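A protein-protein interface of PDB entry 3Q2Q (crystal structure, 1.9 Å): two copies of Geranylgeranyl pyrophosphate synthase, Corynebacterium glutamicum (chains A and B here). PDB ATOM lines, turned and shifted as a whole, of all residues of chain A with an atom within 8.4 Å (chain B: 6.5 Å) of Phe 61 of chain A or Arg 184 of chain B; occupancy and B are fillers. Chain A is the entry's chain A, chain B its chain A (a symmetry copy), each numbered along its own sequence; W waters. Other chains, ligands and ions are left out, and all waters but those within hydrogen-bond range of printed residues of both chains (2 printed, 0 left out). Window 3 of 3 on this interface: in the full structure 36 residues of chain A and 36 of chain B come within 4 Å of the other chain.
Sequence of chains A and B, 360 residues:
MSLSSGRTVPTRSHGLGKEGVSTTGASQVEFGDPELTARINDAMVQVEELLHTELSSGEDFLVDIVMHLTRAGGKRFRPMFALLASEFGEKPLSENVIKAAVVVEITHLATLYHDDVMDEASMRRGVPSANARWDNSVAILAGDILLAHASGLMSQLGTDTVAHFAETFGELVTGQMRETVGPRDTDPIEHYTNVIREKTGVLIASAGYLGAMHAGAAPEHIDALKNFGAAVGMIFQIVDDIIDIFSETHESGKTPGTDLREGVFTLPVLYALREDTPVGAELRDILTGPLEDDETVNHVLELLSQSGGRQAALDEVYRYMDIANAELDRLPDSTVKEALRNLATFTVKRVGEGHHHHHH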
ATOM      1  N   GLY A  58      21.453 -13.567 -19.424  1.00  0.00           N
ATOM      2  CA  GLY A  58      21.462 -14.583 -20.487  1.00  0.00           C
ATOM      3  C   GLY A  58      22.860 -15.041 -20.839  1.00  0.00           C
ATOM      4  O   GLY A  58      23.851 -14.627 -20.219  1.00  0.00           O
ATOM      5  N   GLU A  59      22.938 -15.878 -21.868  1.00  0.00           N
ATOM      6  CA  GLU A  59      24.189 -16.514 -22.251  1.00  0.00           C
ATOM      7  C   GLU A  59      25.149 -15.460 -22.748  1.00  0.00           C
ATOM      8  O   GLU A  59      24.733 -14.472 -23.362  1.00  0.00           O
ATOM      9  CB  GLU A  59      23.937 -17.525 -23.384  1.00  0.00           C
ATOM     10  CG  GLU A  59      23.149 -18.746 -22.929  1.00  0.00           C
ATOM     11  CD  GLU A  59      23.988 -19.681 -22.098  1.00  0.00           C
ATOM     12  OE1 GLU A  59      25.227 -19.500 -22.049  1.00  0.00           O
ATOM     13  OE2 GLU A  59      23.418 -20.598 -21.486  1.00  0.00           O
ATOM     14  N   ASP A  60      26.428 -15.680 -22.484  1.00  0.00           N
ATOM     15  CA  ASP A  60      27.458 -14.728 -22.917  1.00  0.00           C
ATOM     16  C   ASP A  60      27.305 -14.250 -24.356  1.00  0.00           C
ATOM     17  O   ASP A  60      27.337 -13.049 -24.619  1.00  0.00           O
ATOM     18  CB  ASP A  60      28.882 -15.261 -22.621  1.00  0.00           C
ATOM     19  CG  ASP A  60      29.194 -16.632 -23.267  1.00  0.00           C
ATOM     20  OD1 ASP A  60      28.329 -17.279 -23.902  1.00  0.00           O
ATOM     21  OD2 ASP A  60      30.354 -17.072 -23.112  1.00  0.00           O
ATOM     22  N   PHE A  61      27.108 -15.171 -25.301  1.00  0.00           N
ATOM     23  CA  PHE A  61      27.093 -14.773 -26.716  1.00  0.00           C
ATOM     24  C   PHE A  61      25.903 -13.882 -27.031  1.00  0.00           C
ATOM     25  O   PHE A  61      25.954 -13.036 -27.918  1.00  0.00           O
ATOM     26  CB  PHE A  61      27.100 -16.005 -27.651  1.00  0.00           C
ATOM     27  CG  PHE A  61      25.981 -16.975 -27.367  1.00  0.00           C
ATOM     28  CD1 PHE A  61      24.711 -16.768 -27.912  1.00  0.00           C
ATOM     29  CD2 PHE A  61      26.197 -18.066 -26.540  1.00  0.00           C
ATOM     30  CE1 PHE A  61      23.664 -17.640 -27.629  1.00  0.00           C
ATOM     31  CE2 PHE A  61      25.167 -18.960 -26.244  1.00  0.00           C
ATOM     32  CZ  PHE A  61      23.898 -18.738 -26.786  1.00  0.00           C
ATOM     33  N   LEU A  62      24.816 -14.066 -26.292  1.00  0.00           N
ATOM     34  CA  LEU A  62      23.626 -13.255 -26.489  1.00  0.00           C
ATOM     35  C   LEU A  62      23.776 -11.872 -25.832  1.00  0.00           C
ATOM     36  O   LEU A  62      23.447 -10.831 -26.429  1.00  0.00           O
ATOM     37  CB  LEU A  62      22.414 -14.009 -25.911  1.00  0.00           C
ATOM     38  CG  LEU A  62      21.090 -13.282 -26.028  1.00  0.00           C
ATOM     39  CD1 LEU A  62      19.967 -14.279 -26.249  1.00  0.00           C
ATOM     40  CD2 LEU A  62      20.888 -12.529 -24.701  1.00  0.00           C
ATOM     41  N   VAL A  63      24.287 -11.861 -24.609  1.00  0.00           N
ATOM     42  CA  VAL A  63      24.505 -10.589 -23.913  1.00  0.00           C
ATOM     43  C   VAL A  63      25.470  -9.702 -24.707  1.00  0.00           C
ATOM     44  O   VAL A  63      25.224  -8.508 -24.905  1.00  0.00           O
ATOM     45  CB  VAL A  63      25.025 -10.822 -22.492  1.00  0.00           C
ATOM     46  CG1 VAL A  63      25.417  -9.504 -21.857  1.00  0.00           C
ATOM     47  CG2 VAL A  63      23.939 -11.515 -21.671  1.00  0.00           C
ATOM     48  N   ASP A  64      26.553 -10.293 -25.188  1.00  0.00           N
ATOM     49  CA  ASP A  64      27.504  -9.567 -26.022  1.00  0.00           C
ATOM     50  C   ASP A  64      26.787  -8.838 -27.156  1.00  0.00           C
ATOM     51  O   ASP A  64      27.055  -7.669 -27.432  1.00  0.00           O
ATOM     52  CB  ASP A  64      28.550 -10.525 -26.589  1.00  0.00           C
ATOM     53  CG  ASP A  64      29.559  -9.828 -27.470  1.00  0.00           C
ATOM     54  OD1 ASP A  64      29.684 -10.214 -28.652  1.00  0.00           O
ATOM     55  OD2 ASP A  64      30.224  -8.889 -26.981  1.00  0.00           O
ATOM     56  N   ILE A  65      25.861  -9.531 -27.817  1.00  0.00           N
ATOM     57  CA  ILE A  65      25.132  -8.907 -28.922  1.00  0.00           C
ATOM     58  C   ILE A  65      24.212  -7.775 -28.466  1.00  0.00           C
ATOM     59  O   ILE A  65      24.169  -6.712 -29.085  1.00  0.00           O
ATOM     60  CB  ILE A  65      24.343  -9.938 -29.736  1.00  0.00           C
ATOM     61  CG1 ILE A  65      25.306 -10.744 -30.613  1.00  0.00           C
ATOM     62  CG2 ILE A  65      23.274  -9.251 -30.570  1.00  0.00           C
ATOM     63  CD1 ILE A  65      24.778 -12.104 -30.993  1.00  0.00           C
ATOM     64  N   VAL A  66      23.478  -8.000 -27.381  1.00  0.00           N
ATOM     65  CA  VAL A  66      22.579  -6.983 -26.857  1.00  0.00           C
ATOM     66  C   VAL A  66      23.397  -5.765 -26.431  1.00  0.00           C
ATOM     67  O   VAL A  66      23.023  -4.628 -26.723  1.00  0.00           O
ATOM     68  CB  VAL A  66      21.759  -7.506 -25.627  1.00  0.00           C
ATOM     69  CG1 VAL A  66      21.086  -6.342 -24.890  1.00  0.00           C
ATOM     70  CG2 VAL A  66      20.717  -8.540 -26.074  1.00  0.00           C
ATOM     71  N   MET A  67      24.520  -5.991 -25.749  1.00  0.00           N
ATOM     72  CA  MET A  67      25.275  -4.842 -25.277  1.00  0.00           C
ATOM     73  C   MET A  67      25.869  -4.055 -26.453  1.00  0.00           C
ATOM     74  O   MET A  67      25.869  -2.823 -26.412  1.00  0.00           O
ATOM     75  CB  MET A  67      26.308  -5.226 -24.209  1.00  0.00           C
ATOM     76  CG  MET A  67      25.687  -5.874 -22.946  1.00  0.00           C
ATOM     77  SD  MET A  67      25.027  -4.794 -21.631  1.00  0.00           S
ATOM     78  CE  MET A  67      23.763  -3.869 -22.489  1.00  0.00           C
ATOM     79  N   HIS A  68      26.301  -4.741 -27.506  1.00  0.00           N
ATOM     80  CA  HIS A  68      26.826  -4.051 -28.683  1.00  0.00           C
ATOM     81  C   HIS A  68      25.763  -3.223 -29.404  1.00  0.00           C
ATOM     82  O   HIS A  68      26.078  -2.208 -30.027  1.00  0.00           O
ATOM     83  CB  HIS A  68      27.494  -5.031 -29.654  1.00  0.00           C
ATOM     84  CG  HIS A  68      28.917  -5.351 -29.308  1.00  0.00           C
ATOM     85  ND1 HIS A  68      29.857  -4.378 -29.043  1.00  0.00           N
ATOM     86  CD2 HIS A  68      29.565  -6.537 -29.203  1.00  0.00           C
ATOM     87  CE1 HIS A  68      31.019  -4.950 -28.778  1.00  0.00           C
ATOM     88  NE2 HIS A  68      30.869  -6.259 -28.869  1.00  0.00           N
ATOM     89  N   TRP A 134      22.847 -10.830 -41.450  1.00  0.00           N
ATOM     90  CA  TRP A 134      23.256 -11.245 -40.122  1.00  0.00           C
ATOM     91  C   TRP A 134      22.875 -10.152 -39.123  1.00  0.00           C
ATOM     92  O   TRP A 134      22.312 -10.436 -38.064  1.00  0.00           O
ATOM     93  CB  TRP A 134      24.763 -11.521 -40.083  1.00  0.00           C
ATOM     94  CG  TRP A 134      25.244 -12.076 -38.771  1.00  0.00           C
ATOM     95  CD1 TRP A 134      25.315 -13.395 -38.412  1.00  0.00           C
ATOM     96  CD2 TRP A 134      25.717 -11.326 -37.641  1.00  0.00           C
ATOM     97  NE1 TRP A 134      25.803 -13.510 -37.129  1.00  0.00           N
ATOM     98  CE2 TRP A 134      26.056 -12.256 -36.634  1.00  0.00           C
ATOM     99  CE3 TRP A 134      25.883  -9.961 -37.383  1.00  0.00           C
ATOM    100  CZ2 TRP A 134      26.553 -11.863 -35.390  1.00  0.00           C
ATOM    101  CZ3 TRP A 134      26.374  -9.572 -36.147  1.00  0.00           C
ATOM    102  CH2 TRP A 134      26.703 -10.519 -35.167  1.00  0.00           C
ATOM    103  N   VAL A 138      20.123 -10.468 -35.988  1.00  0.00           N
ATOM    104  CA  VAL A 138      20.634 -10.200 -34.665  1.00  0.00           C
ATOM    105  C   VAL A 138      19.723  -9.227 -33.916  1.00  0.00           C
ATOM    106  O   VAL A 138      19.364  -9.478 -32.762  1.00  0.00           O
ATOM    107  CB  VAL A 138      22.126  -9.760 -34.734  1.00  0.00           C
ATOM    108  CG1 VAL A 138      22.422  -8.603 -33.808  1.00  0.00           C
ATOM    109  CG2 VAL A 138      23.025 -10.944 -34.429  1.00  0.00           C
ATOM    110  N   VAL B 173      14.567 -18.101 -27.913  1.00  0.00           N
ATOM    111  CA  VAL B 173      15.308 -17.024 -28.548  1.00  0.00           C
ATOM    112  C   VAL B 173      16.821 -17.226 -28.403  1.00  0.00           C
ATOM    113  O   VAL B 173      17.572 -16.962 -29.333  1.00  0.00           O
ATOM    114  CB  VAL B 173      14.923 -15.625 -27.988  1.00  0.00           C
ATOM    115  CG1 VAL B 173      15.857 -14.541 -28.565  1.00  0.00           C
ATOM    116  CG2 VAL B 173      13.451 -15.308 -28.301  1.00  0.00           C
ATOM    117  N   THR B 174      17.255 -17.702 -27.238  1.00  0.00           N
ATOM    118  CA  THR B 174      18.646 -18.063 -27.032  1.00  0.00           C
ATOM    119  C   THR B 174      19.111 -19.115 -28.054  1.00  0.00           C
ATOM    120  O   THR B 174      20.202 -18.986 -28.611  1.00  0.00           O
ATOM    121  CB  THR B 174      18.908 -18.493 -25.587  1.00  0.00           C
ATOM    122  OG1 THR B 174      18.583 -17.387 -24.719  1.00  0.00           O
ATOM    123  CG2 THR B 174      20.378 -18.911 -25.385  1.00  0.00           C
ATOM    124  N   GLY B 175      18.281 -20.125 -28.327  1.00  0.00           N
ATOM    125  CA  GLY B 175      18.625 -21.144 -29.318  1.00  0.00           C
ATOM    126  C   GLY B 175      18.797 -20.580 -30.721  1.00  0.00           C
ATOM    127  O   GLY B 175      19.746 -20.947 -31.438  1.00  0.00           O
ATOM    128  N   MET B 177      19.598 -17.464 -31.403  1.00  0.00           N
ATOM    129  CA  MET B 177      20.836 -16.650 -31.376  1.00  0.00           C
ATOM    130  C   MET B 177      22.066 -17.547 -31.438  1.00  0.00           C
ATOM    131  O   MET B 177      23.032 -17.242 -32.147  1.00  0.00           O
ATOM    132  CB  MET B 177      20.920 -15.757 -30.118  1.00  0.00           C
ATOM    133  CG  MET B 177      22.013 -14.665 -30.181  1.00  0.00           C
ATOM    134  SD  MET B 177      21.726 -13.312 -31.380  1.00  0.00           S
ATOM    135  CE  MET B 177      20.770 -12.168 -30.374  1.00  0.00           C
ATOM    136  N   ARG B 178      22.019 -18.644 -30.687  1.00  0.00           N
ATOM    137  CA  ARG B 178      23.125 -19.600 -30.608  1.00  0.00           C
ATOM    138  C   ARG B 178      23.425 -20.183 -31.980  1.00  0.00           C
ATOM    139  O   ARG B 178      24.580 -20.289 -32.396  1.00  0.00           O
ATOM    140  CB  ARG B 178      22.794 -20.734 -29.625  1.00  0.00           C
ATOM    141  CG  ARG B 178      23.966 -21.687 -29.383  1.00  0.00           C
ATOM    142  CD  ARG B 178      23.640 -22.859 -28.489  1.00  0.00           C
ATOM    143  NE  ARG B 178      23.163 -22.492 -27.157  1.00  0.00           N
ATOM    144  CZ  ARG B 178      23.938 -22.328 -26.087  1.00  0.00           C
ATOM    145  NH1 ARG B 178      25.251 -22.477 -26.181  1.00  0.00           N
ATOM    146  NH2 ARG B 178      23.392 -22.027 -24.921  1.00  0.00           N
ATOM    147  N   GLU B 179      22.375 -20.565 -32.686  1.00  0.00           N
ATOM    148  CA  GLU B 179      22.538 -21.085 -34.035  1.00  0.00           C
ATOM    149  C   GLU B 179      23.127 -20.017 -34.964  1.00  0.00           C
ATOM    150  O   GLU B 179      23.969 -20.310 -35.811  1.00  0.00           O
ATOM    151  CB  GLU B 179      21.192 -21.548 -34.579  1.00  0.00           C
ATOM    152  CG  GLU B 179      21.291 -22.260 -35.917  1.00  0.00           C
ATOM    153  CD  GLU B 179      19.927 -22.663 -36.425  1.00  0.00           C
ATOM    154  OE1 GLU B 179      18.978 -21.861 -36.271  1.00  0.00           O
ATOM    155  OE2 GLU B 179      19.799 -23.780 -36.964  1.00  0.00           O
ATOM    156  N   VAL B 181      25.068 -17.364 -34.203  1.00  0.00           N
ATOM    157  CA  VAL B 181      26.474 -17.043 -33.929  1.00  0.00           C
ATOM    158  C   VAL B 181      27.428 -18.208 -34.167  1.00  0.00           C
ATOM    159  O   VAL B 181      28.619 -17.998 -34.388  1.00  0.00           O
ATOM    160  CB  VAL B 181      26.709 -16.519 -32.480  1.00  0.00           C
ATOM    161  CG1 VAL B 181      25.801 -15.325 -32.172  1.00  0.00           C
ATOM    162  CG2 VAL B 181      26.540 -17.633 -31.455  1.00  0.00           C
ATOM    163  N   GLY B 182      26.921 -19.435 -34.104  1.00  0.00           N
ATOM    164  CA  GLY B 182      27.777 -20.595 -34.274  1.00  0.00           C
ATOM    165  C   GLY B 182      28.469 -21.064 -33.009  1.00  0.00           C
ATOM    166  O   GLY B 182      28.326 -20.452 -31.951  1.00  0.00           O
ATOM    167  N   PRO B 183      29.246 -22.153 -33.117  1.00  0.00           N
ATOM    168  CA  PRO B 183      29.873 -22.813 -31.966  1.00  0.00           C
ATOM    169  C   PRO B 183      31.087 -22.088 -31.370  1.00  0.00           C
ATOM    170  O   PRO B 183      31.637 -22.555 -30.371  1.00  0.00           O
ATOM    171  CB  PRO B 183      30.282 -24.188 -32.514  1.00  0.00           C
ATOM    172  CG  PRO B 183      30.423 -23.984 -34.010  1.00  0.00           C
ATOM    173  CD  PRO B 183      29.434 -22.899 -34.380  1.00  0.00           C
ATOM    174  N   ARG B 184      31.472 -20.953 -31.949  1.00  0.00           N
ATOM    175  CA  ARG B 184      32.683 -20.238 -31.515  1.00  0.00           C
ATOM    176  C   ARG B 184      33.829 -21.241 -31.385  1.00  0.00           C
ATOM    177  O   ARG B 184      34.291 -21.801 -32.380  1.00  0.00           O
ATOM    178  CB  ARG B 184      32.465 -19.511 -30.178  1.00  0.00           C
ATOM    179  CG  ARG B 184      31.687 -18.192 -30.250  1.00  0.00           C
ATOM    180  CD  ARG B 184      30.648 -18.142 -29.128  1.00  0.00           C
ATOM    181  NE  ARG B 184      29.620 -19.143 -29.385  1.00  0.00           N
ATOM    182  CZ  ARG B 184      29.069 -19.935 -28.470  1.00  0.00           C
ATOM    183  NH1 ARG B 184      28.153 -20.815 -28.850  1.00  0.00           N
ATOM    184  NH2 ARG B 184      29.430 -19.862 -27.192  1.00  0.00           N
ATOM    185  N   ASP B 185      34.268 -21.480 -30.155  1.00  0.00           N
ATOM    186  CA  ASP B 185      35.336 -22.433 -29.911  1.00  0.00           C
ATOM    187  C   ASP B 185      34.906 -23.531 -28.951  1.00  0.00           C
ATOM    188  O   ASP B 185      35.745 -24.148 -28.296  1.00  0.00           O
ATOM    189  CB  ASP B 185      36.578 -21.717 -29.365  1.00  0.00           C
ATOM    190  CG  ASP B 185      37.288 -20.890 -30.426  1.00  0.00           C
ATOM    191  OD1 ASP B 185      36.984 -21.067 -31.628  1.00  0.00           O
ATOM    192  OD2 ASP B 185      38.155 -20.064 -30.057  1.00  0.00           O
ATOM    193  N   THR B 186      33.601 -23.778 -28.862  1.00  0.00           N
ATOM    194  CA  THR B 186      33.106 -24.893 -28.055  1.00  0.00           C
ATOM    195  C   THR B 186      33.017 -26.167 -28.897  1.00  0.00           C
ATOM    196  O   THR B 186      33.059 -26.122 -30.134  1.00  0.00           O
ATOM    197  CB  THR B 186      31.715 -24.595 -27.466  1.00  0.00           C
ATOM    198  OG1 THR B 186      30.796 -24.331 -28.529  1.00  0.00           O
ATOM    199  CG2 THR B 186      31.772 -23.383 -26.535  1.00  0.00           C
ATOM    200  N   HIS B 191      27.415 -27.822 -28.952  1.00  0.00           N
ATOM    201  CA  HIS B 191      26.728 -26.703 -29.573  1.00  0.00           C
ATOM    202  C   HIS B 191      25.433 -27.191 -30.229  1.00  0.00           C
ATOM    203  O   HIS B 191      24.349 -26.646 -30.021  1.00  0.00           O
ATOM    204  CB  HIS B 191      27.642 -26.073 -30.635  1.00  0.00           C
ATOM    205  CG  HIS B 191      26.980 -25.035 -31.485  1.00  0.00           C
ATOM    206  ND1 HIS B 191      26.680 -23.769 -31.023  1.00  0.00           N
ATOM    207  CD2 HIS B 191      26.586 -25.063 -32.781  1.00  0.00           C
ATOM    208  CE1 HIS B 191      26.119 -23.071 -31.993  1.00  0.00           C
ATOM    209  NE2 HIS B 191      26.051 -23.832 -33.071  1.00  0.00           N
ATOM    210  N   GLU B 198      17.243 -25.918 -27.051  1.00  0.00           N
ATOM    211  CA  GLU B 198      16.695 -24.567 -26.897  1.00  0.00           C
ATOM    212  C   GLU B 198      15.706 -24.168 -27.981  1.00  0.00           C
ATOM    213  O   GLU B 198      14.621 -23.660 -27.678  1.00  0.00           O
ATOM    214  CB  GLU B 198      17.835 -23.525 -26.824  1.00  0.00           C
ATOM    215  CG  GLU B 198      18.651 -23.629 -25.524  1.00  0.00           C
ATOM    216  CD  GLU B 198      19.975 -22.898 -25.591  1.00  0.00           C
ATOM    217  OE1 GLU B 198      20.327 -22.437 -26.682  1.00  0.00           O
ATOM    218  OE2 GLU B 198      20.678 -22.798 -24.559  1.00  0.00           O
HETATM  219  O   HOH W   1      25.402 -22.689 -22.548  1.00  0.00           O
HETATM  220  O   HOH W   2      20.090 -16.551 -22.685  1.00  0.00           O
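The guanidinium group (NH2) of Arg 178 of chain B lies within salt-bridge range of the side-chain carboxylate (OE2) of Glu 59 of chain A (3.7 Å).
The side-chain carboxylate (OE2) of Glu 198 of chain B is in salt-bridge range of the guanidinium group (NH2) of Arg 178 of chain B (2.8 Å).
The backbone carbonyl oxygen (O) of Gly 182 of chain B is in hydrogen-bond range of the guanidinium group (NH1) of Arg 184 of chain B, at 3.1 Å.
Glu 59 of chain A touches Thr 174 of chain B.
Phe 61 of chain A touches Thr 174 of chain B.
CE2 of Phe 61 of chain A touches NH1 of Arg 178 of chain B, at 3.5 Å.
Phe 61 of chain A touches Arg 184 of chain B.
Thr 174 of chain B touches Leu 62 of chain A.
CD1 of Ile 65 of chain A touches SD of Met 177 of chain B, 3.3 Å away.
Ile 65 of chain A touches Val 181 of chain B (CD1 to CG1, 3.6 Å).
O of Val 138 of chain A touches CE of Met 177 of chain B (3.9 Å).
Phe 61 of chain A touches three residues of chain B.
Val 66 of chain A touches none of the printed residues of chain B.
Of the printed residues of chain A, Thr 174 of chain B touches Glu 59, Phe 61 and Leu 62.
Of the printed residues of chain A, Val 181 of chain B touches Ile 65 (3.6 Å).
No residue of chain A comes within 4 Å of Pro 183 of chain B.
Arg 184 of chain B touches just one residue of chain A: Phe 61.
Asp 185 of chain B touches none of the printed residues of chain A.
The nearest residue of chain A that does not touch Arg 184 of chain B is Asp 60 of chain A (4.3 Å).
The nearest printed residue of chain B that does not touch Glu 59 of chain A is Glu 198 of chain B (4.7 Å).
Hydrophobic or aromatic side chains of chain A within 4 Å of the printed part of chain B: Phe 61, Leu 62 and Ile 65.
Printed residues of chain B that touch a printed residue of chain A: Thr 174, Met 177, Arg 178, Val 181 and Arg 184.
Hydrophobic or aromatic side chains of chain B within 4 Å of the printed part of chain A: Met 177 and Val 181.
Along chain B the printed residues that touch a printed residue of chain A span positions 174 to 184.
Among the printed residues, 9 pairs touch across the chains.
Among the printed residues, Asp or Glu carboxylates within 4 Å of a Lys or Arg side-chain nitrogen of the other chain: Glu 59 of chain A with Arg 178 of chain B (3.7 Å).
No position is printed for both chains.
Of the 9 pairs that touch across the chains among the printed residues, none has its exchanged pair printed and touching as well.
Water W2 bridges the side-chain hydroxyl of Thr 174 of chain B (2.7 Å) and the backbone NH of Glu 59 of chain A (3.0 Å).
Water W1 lies within hydrogen-bond range of OE2 of Glu 59 of chain A (3.1 Å) and NH2 of Arg 178 of chain B (3.2 Å).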
